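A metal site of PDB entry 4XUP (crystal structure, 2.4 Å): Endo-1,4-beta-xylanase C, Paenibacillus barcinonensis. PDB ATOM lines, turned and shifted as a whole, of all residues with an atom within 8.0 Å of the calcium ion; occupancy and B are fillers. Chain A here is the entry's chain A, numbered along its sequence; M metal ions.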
ATOM      1  N   ALA A 176       3.568  -6.768 -37.034  1.00  0.00           N
ATOM      2  CA  ALA A 176       3.853  -7.891 -36.146  1.00  0.00           C
ATOM      3  C   ALA A 176       4.746  -7.407 -35.006  1.00  0.00           C
ATOM      4  O   ALA A 176       5.890  -7.016 -35.207  1.00  0.00           O
ATOM      5  CB  ALA A 176       4.480  -9.051 -36.891  1.00  0.00           C
ATOM      6  N   ASP A 177       4.165  -7.441 -33.819  1.00  0.00           N
ATOM      7  CA  ASP A 177       4.833  -7.063 -32.567  1.00  0.00           C
ATOM      8  C   ASP A 177       5.056  -8.266 -31.624  1.00  0.00           C
ATOM      9  O   ASP A 177       5.821  -8.176 -30.671  1.00  0.00           O
ATOM     10  CB  ASP A 177       4.082  -5.915 -31.851  1.00  0.00           C
ATOM     11  CG  ASP A 177       2.690  -6.316 -31.340  1.00  0.00           C
ATOM     12  OD1 ASP A 177       2.401  -7.532 -31.140  1.00  0.00           O
ATOM     13  OD2 ASP A 177       1.869  -5.406 -31.116  1.00  0.00           O
ATOM     14  N   PHE A 178       4.363  -9.363 -31.903  1.00  0.00           N
ATOM     15  CA  PHE A 178       4.489 -10.665 -31.191  1.00  0.00           C
ATOM     16  C   PHE A 178       3.990 -10.664 -29.750  1.00  0.00           C
ATOM     17  O   PHE A 178       4.228 -11.630 -29.020  1.00  0.00           O
ATOM     18  CB  PHE A 178       5.950 -11.211 -31.263  1.00  0.00           C
ATOM     19  CG  PHE A 178       6.445 -11.333 -32.664  1.00  0.00           C
ATOM     20  CD1 PHE A 178       5.925 -12.326 -33.523  1.00  0.00           C
ATOM     21  CD2 PHE A 178       7.357 -10.407 -33.176  1.00  0.00           C
ATOM     22  CE1 PHE A 178       6.327 -12.397 -34.842  1.00  0.00           C
ATOM     23  CE2 PHE A 178       7.788 -10.490 -34.498  1.00  0.00           C
ATOM     24  CZ  PHE A 178       7.279 -11.487 -35.328  1.00  0.00           C
ATOM     25  N   GLU A 179       3.337  -9.586 -29.342  1.00  0.00           N
ATOM     26  CA  GLU A 179       2.941  -9.402 -27.920  1.00  0.00           C
ATOM     27  C   GLU A 179       1.826 -10.366 -27.489  1.00  0.00           C
ATOM     28  O   GLU A 179       1.750 -10.789 -26.342  1.00  0.00           O
ATOM     29  CB  GLU A 179       2.563  -7.948 -27.626  1.00  0.00           C
ATOM     30  CG  GLU A 179       3.714  -6.957 -27.810  1.00  0.00           C
ATOM     31  CD  GLU A 179       5.004  -7.354 -27.070  1.00  0.00           C
ATOM     32  OE1 GLU A 179       4.944  -7.780 -25.885  1.00  0.00           O
ATOM     33  OE2 GLU A 179       6.095  -7.240 -27.681  1.00  0.00           O
ATOM     34  N   ASP A 180       0.994 -10.725 -28.453  1.00  0.00           N
ATOM     35  CA  ASP A 180      -0.055 -11.763 -28.262  1.00  0.00           C
ATOM     36  C   ASP A 180       0.498 -13.197 -28.095  1.00  0.00           C
ATOM     37  O   ASP A 180      -0.278 -14.151 -27.995  1.00  0.00           O
ATOM     38  CB  ASP A 180      -1.115 -11.698 -29.387  1.00  0.00           C
ATOM     39  CG  ASP A 180      -0.545 -11.929 -30.812  1.00  0.00           C
ATOM     40  OD1 ASP A 180       0.603 -12.402 -30.993  1.00  0.00           O
ATOM     41  OD2 ASP A 180      -1.277 -11.606 -31.774  1.00  0.00           O
ATOM     42  N   VAL A 196       8.373 -17.732 -30.375  1.00  0.00           N
ATOM     43  CA  VAL A 196       8.038 -16.421 -29.816  1.00  0.00           C
ATOM     44  C   VAL A 196       8.474 -16.465 -28.383  1.00  0.00           C
ATOM     45  O   VAL A 196       7.924 -17.196 -27.585  1.00  0.00           O
ATOM     46  CB  VAL A 196       6.549 -16.063 -29.878  1.00  0.00           C
ATOM     47  CG1 VAL A 196       6.325 -14.692 -29.245  1.00  0.00           C
ATOM     48  CG2 VAL A 196       6.071 -16.018 -31.321  1.00  0.00           C
ATOM     49  N   VAL A 197       9.493 -15.691 -28.072  1.00  0.00           N
ATOM     50  CA  VAL A 197      10.000 -15.666 -26.684  1.00  0.00           C
ATOM     51  C   VAL A 197       9.328 -14.543 -25.904  1.00  0.00           C
ATOM     52  O   VAL A 197       8.899 -13.537 -26.477  1.00  0.00           O
ATOM     53  CB  VAL A 197      11.547 -15.550 -26.576  1.00  0.00           C
ATOM     54  CG1 VAL A 197      12.199 -16.814 -27.089  1.00  0.00           C
ATOM     55  CG2 VAL A 197      12.093 -14.328 -27.294  1.00  0.00           C
ATOM     56  N   ILE A 200      12.190 -10.963 -23.809  1.00  0.00           N
ATOM     57  CA  ILE A 200      13.092 -10.314 -24.795  1.00  0.00           C
ATOM     58  C   ILE A 200      12.265  -9.687 -25.916  1.00  0.00           C
ATOM     59  O   ILE A 200      11.432 -10.323 -26.536  1.00  0.00           O
ATOM     60  CB  ILE A 200      14.128 -11.271 -25.429  1.00  0.00           C
ATOM     61  CG1 ILE A 200      14.962 -11.948 -24.337  1.00  0.00           C
ATOM     62  CG2 ILE A 200      15.027 -10.519 -26.422  1.00  0.00           C
ATOM     63  CD1 ILE A 200      16.018 -12.928 -24.823  1.00  0.00           C
ATOM     64  N   GLY A 201      12.586  -8.445 -26.212  1.00  0.00           N
ATOM     65  CA  GLY A 201      11.881  -7.672 -27.212  1.00  0.00           C
ATOM     66  C   GLY A 201      12.361  -6.250 -27.357  1.00  0.00           C
ATOM     67  O   GLY A 201      13.133  -5.762 -26.549  1.00  0.00           O
ATOM     68  N   HIS A 202      11.926  -5.618 -28.434  1.00  0.00           N
ATOM     69  CA  HIS A 202      12.263  -4.236 -28.769  1.00  0.00           C
ATOM     70  C   HIS A 202      11.268  -3.296 -28.110  1.00  0.00           C
ATOM     71  O   HIS A 202      10.136  -3.168 -28.583  1.00  0.00           O
ATOM     72  CB  HIS A 202      12.271  -3.999 -30.264  1.00  0.00           C
ATOM     73  CG  HIS A 202      12.485  -2.554 -30.644  1.00  0.00           C
ATOM     74  ND1 HIS A 202      13.578  -1.830 -30.249  1.00  0.00           N
ATOM     75  CD2 HIS A 202      11.746  -1.726 -31.419  1.00  0.00           C
ATOM     76  CE1 HIS A 202      13.517  -0.619 -30.769  1.00  0.00           C
ATOM     77  NE2 HIS A 202      12.420  -0.530 -31.483  1.00  0.00           N
ATOM     78  N   ASN A 203      11.732  -2.651 -27.037  1.00  0.00           N
ATOM     79  CA  ASN A 203      10.874  -1.800 -26.170  1.00  0.00           C
ATOM     80  C   ASN A 203       9.561  -2.524 -25.845  1.00  0.00           C
ATOM     81  O   ASN A 203       8.453  -1.986 -25.976  1.00  0.00           O
ATOM     82  CB  ASN A 203      10.607  -0.433 -26.809  1.00  0.00           C
ATOM     83  CG  ASN A 203      11.881   0.390 -26.999  1.00  0.00           C
ATOM     84  OD1 ASN A 203      12.000   1.118 -27.972  1.00  0.00           O
ATOM     85  ND2 ASN A 203      12.822   0.300 -26.058  1.00  0.00           N
ATOM     86  N   SER A 204       9.718  -3.785 -25.457  1.00  0.00           N
ATOM     87  CA  SER A 204       8.603  -4.711 -25.332  1.00  0.00           C
ATOM     88  C   SER A 204       9.043  -6.057 -24.780  1.00  0.00           C
ATOM     89  O   SER A 204      10.220  -6.370 -24.762  1.00  0.00           O
ATOM     90  CB  SER A 204       7.915  -4.924 -26.701  1.00  0.00           C
ATOM     91  OG  SER A 204       8.800  -5.460 -27.673  1.00  0.00           O
ATOM     92  N   ASN A 205       8.057  -6.836 -24.395  1.00  0.00           N
ATOM     93  CA  ASN A 205       8.267  -8.124 -23.736  1.00  0.00           C
ATOM     94  C   ASN A 205       8.572  -9.318 -24.658  1.00  0.00           C
ATOM     95  O   ASN A 205       9.286 -10.258 -24.286  1.00  0.00           O
ATOM     96  CB  ASN A 205       7.050  -8.475 -22.880  1.00  0.00           C
ATOM     97  CG  ASN A 205       7.401  -9.493 -21.803  1.00  0.00           C
ATOM     98  OD1 ASN A 205       8.346  -9.283 -21.021  1.00  0.00           O
ATOM     99  ND2 ASN A 205       6.706 -10.621 -21.788  1.00  0.00           N
ATOM    100  N   ARG A 206       8.037  -9.263 -25.866  1.00  0.00           N
ATOM    101  CA  ARG A 206       8.129 -10.379 -26.827  1.00  0.00           C
ATOM    102  C   ARG A 206       8.661 -10.048 -28.200  1.00  0.00           C
ATOM    103  O   ARG A 206       8.473  -8.968 -28.734  1.00  0.00           O
ATOM    104  CB  ARG A 206       6.789 -11.066 -27.017  1.00  0.00           C
ATOM    105  CG  ARG A 206       6.098 -11.383 -25.728  1.00  0.00           C
ATOM    106  CD  ARG A 206       5.210 -12.591 -25.852  1.00  0.00           C
ATOM    107  NE  ARG A 206       4.069 -12.558 -24.930  1.00  0.00           N
ATOM    108  CZ  ARG A 206       3.534 -13.604 -24.303  1.00  0.00           C
ATOM    109  NH1 ARG A 206       4.037 -14.830 -24.446  1.00  0.00           N
ATOM    110  NH2 ARG A 206       2.480 -13.415 -23.502  1.00  0.00           N
ATOM    111  N   SER A 207       9.266 -11.074 -28.768  1.00  0.00           N
ATOM    112  CA  SER A 207       9.893 -11.033 -30.081  1.00  0.00           C
ATOM    113  C   SER A 207      10.028 -12.455 -30.648  1.00  0.00           C
ATOM    114  O   SER A 207       9.825 -13.464 -29.960  1.00  0.00           O
ATOM    115  CB  SER A 207      11.274 -10.398 -30.024  1.00  0.00           C
ATOM    116  OG  SER A 207      12.119 -11.101 -29.137  1.00  0.00           O
ATOM    117  N   LEU A 208      10.372 -12.486 -31.927  1.00  0.00           N
ATOM    118  CA  LEU A 208      10.446 -13.720 -32.674  1.00  0.00           C
ATOM    119  C   LEU A 208      11.890 -14.160 -32.782  1.00  0.00           C
ATOM    120  O   LEU A 208      12.704 -13.572 -33.511  1.00  0.00           O
ATOM    121  CB  LEU A 208       9.828 -13.596 -34.059  1.00  0.00           C
ATOM    122  CG  LEU A 208       9.844 -14.879 -34.915  1.00  0.00           C
ATOM    123  CD1 LEU A 208       9.132 -16.044 -34.215  1.00  0.00           C
ATOM    124  CD2 LEU A 208       9.179 -14.636 -36.260  1.00  0.00           C
ATOM    125  N   TRP A 281      19.523  -3.580 -30.431  1.00  0.00           N
ATOM    126  CA  TRP A 281      18.465  -3.567 -31.438  1.00  0.00           C
ATOM    127  C   TRP A 281      18.737  -2.503 -32.491  1.00  0.00           C
ATOM    128  O   TRP A 281      19.152  -1.380 -32.189  1.00  0.00           O
ATOM    129  CB  TRP A 281      17.105  -3.279 -30.814  1.00  0.00           C
ATOM    130  CG  TRP A 281      16.587  -4.386 -29.971  1.00  0.00           C
ATOM    131  CD1 TRP A 281      16.721  -4.516 -28.632  1.00  0.00           C
ATOM    132  CD2 TRP A 281      15.792  -5.503 -30.409  1.00  0.00           C
ATOM    133  NE1 TRP A 281      16.077  -5.651 -28.195  1.00  0.00           N
ATOM    134  CE2 TRP A 281      15.494  -6.269 -29.259  1.00  0.00           C
ATOM    135  CE3 TRP A 281      15.327  -5.939 -31.667  1.00  0.00           C
ATOM    136  CZ2 TRP A 281      14.757  -7.441 -29.328  1.00  0.00           C
ATOM    137  CZ3 TRP A 281      14.598  -7.101 -31.732  1.00  0.00           C
ATOM    138  CH2 TRP A 281      14.315  -7.840 -30.560  1.00  0.00           C
ATOM    139  N   VAL A 324      13.796 -11.019 -34.025  1.00  0.00           N
ATOM    140  CA  VAL A 324      13.136 -10.023 -34.824  1.00  0.00           C
ATOM    141  C   VAL A 324      11.886  -9.549 -34.103  1.00  0.00           C
ATOM    142  O   VAL A 324      11.273 -10.286 -33.348  1.00  0.00           O
ATOM    143  CB  VAL A 324      12.815 -10.664 -36.153  1.00  0.00           C
ATOM    144  CG1 VAL A 324      11.720  -9.956 -36.910  1.00  0.00           C
ATOM    145  CG2 VAL A 324      14.083 -10.707 -36.960  1.00  0.00           C
ATOM    146  N   ASP A 325      11.546  -8.290 -34.318  1.00  0.00           N
ATOM    147  CA  ASP A 325      10.404  -7.608 -33.611  1.00  0.00           C
ATOM    148  C   ASP A 325       9.981  -6.347 -34.335  1.00  0.00           C
ATOM    149  O   ASP A 325      10.681  -5.886 -35.242  1.00  0.00           O
ATOM    150  CB  ASP A 325      10.806  -7.223 -32.184  1.00  0.00           C
ATOM    151  CG  ASP A 325       9.622  -6.951 -31.260  1.00  0.00           C
ATOM    152  OD1 ASP A 325       8.452  -7.044 -31.689  1.00  0.00           O
ATOM    153  OD2 ASP A 325       9.860  -6.643 -30.099  1.00  0.00           O
ATOM    154  N   ASP A 326       8.796  -5.857 -33.967  1.00  0.00           N
ATOM    155  CA  ASP A 326       8.162  -4.622 -34.544  1.00  0.00           C
ATOM    156  C   ASP A 326       8.298  -4.565 -36.071  1.00  0.00           C
ATOM    157  O   ASP A 326       8.844  -3.627 -36.670  1.00  0.00           O
ATOM    158  CB  ASP A 326       8.664  -3.351 -33.862  1.00  0.00           C
ATOM    159  CG  ASP A 326       8.237  -3.281 -32.385  1.00  0.00           C
ATOM    160  OD1 ASP A 326       7.309  -4.019 -31.960  1.00  0.00           O
ATOM    161  OD2 ASP A 326       8.813  -2.456 -31.645  1.00  0.00           O
ATOM    162  N   VAL A 327       7.835  -5.651 -36.672  1.00  0.00           N
ATOM    163  CA  VAL A 327       7.831  -5.821 -38.125  1.00  0.00           C
ATOM    164  C   VAL A 327       6.652  -5.037 -38.655  1.00  0.00           C
ATOM    165  O   VAL A 327       5.553  -5.168 -38.143  1.00  0.00           O
ATOM    166  CB  VAL A 327       7.644  -7.277 -38.582  1.00  0.00           C
ATOM    167  CG1 VAL A 327       7.637  -7.395 -40.104  1.00  0.00           C
ATOM    168  CG2 VAL A 327       8.741  -8.148 -38.031  1.00  0.00           C
HETATM  169 CA    CA M   1       7.563  -7.080 -29.394  1.00  0.00          CA
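The calcium ion is bound by O of Arg 206 (2.2 Å), OE2 of Glu 179 (2.3 Å), O of Asp 177 (2.4 Å), OD2 of Asp 325 (2.4 Å), OD1 of Asp 325 (2.5 Å) and OG of Ser 204 (2.7 Å).
The calcium ion has six donor atoms within binding distance.
The side-chain carboxylate of Asp 325 sits close to the backbone NH of His 202 (2.8 Å).
OG of Ser 204 lies close to O of His 202 (2.8 Å).
Within 4 Å of the calcium ion: Asp 177, Glu 179, Ser 204, Arg 206 and Asp 325.
The nearest printed residue that does not touch the calcium ion is Asp 326 (4.002 Å).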
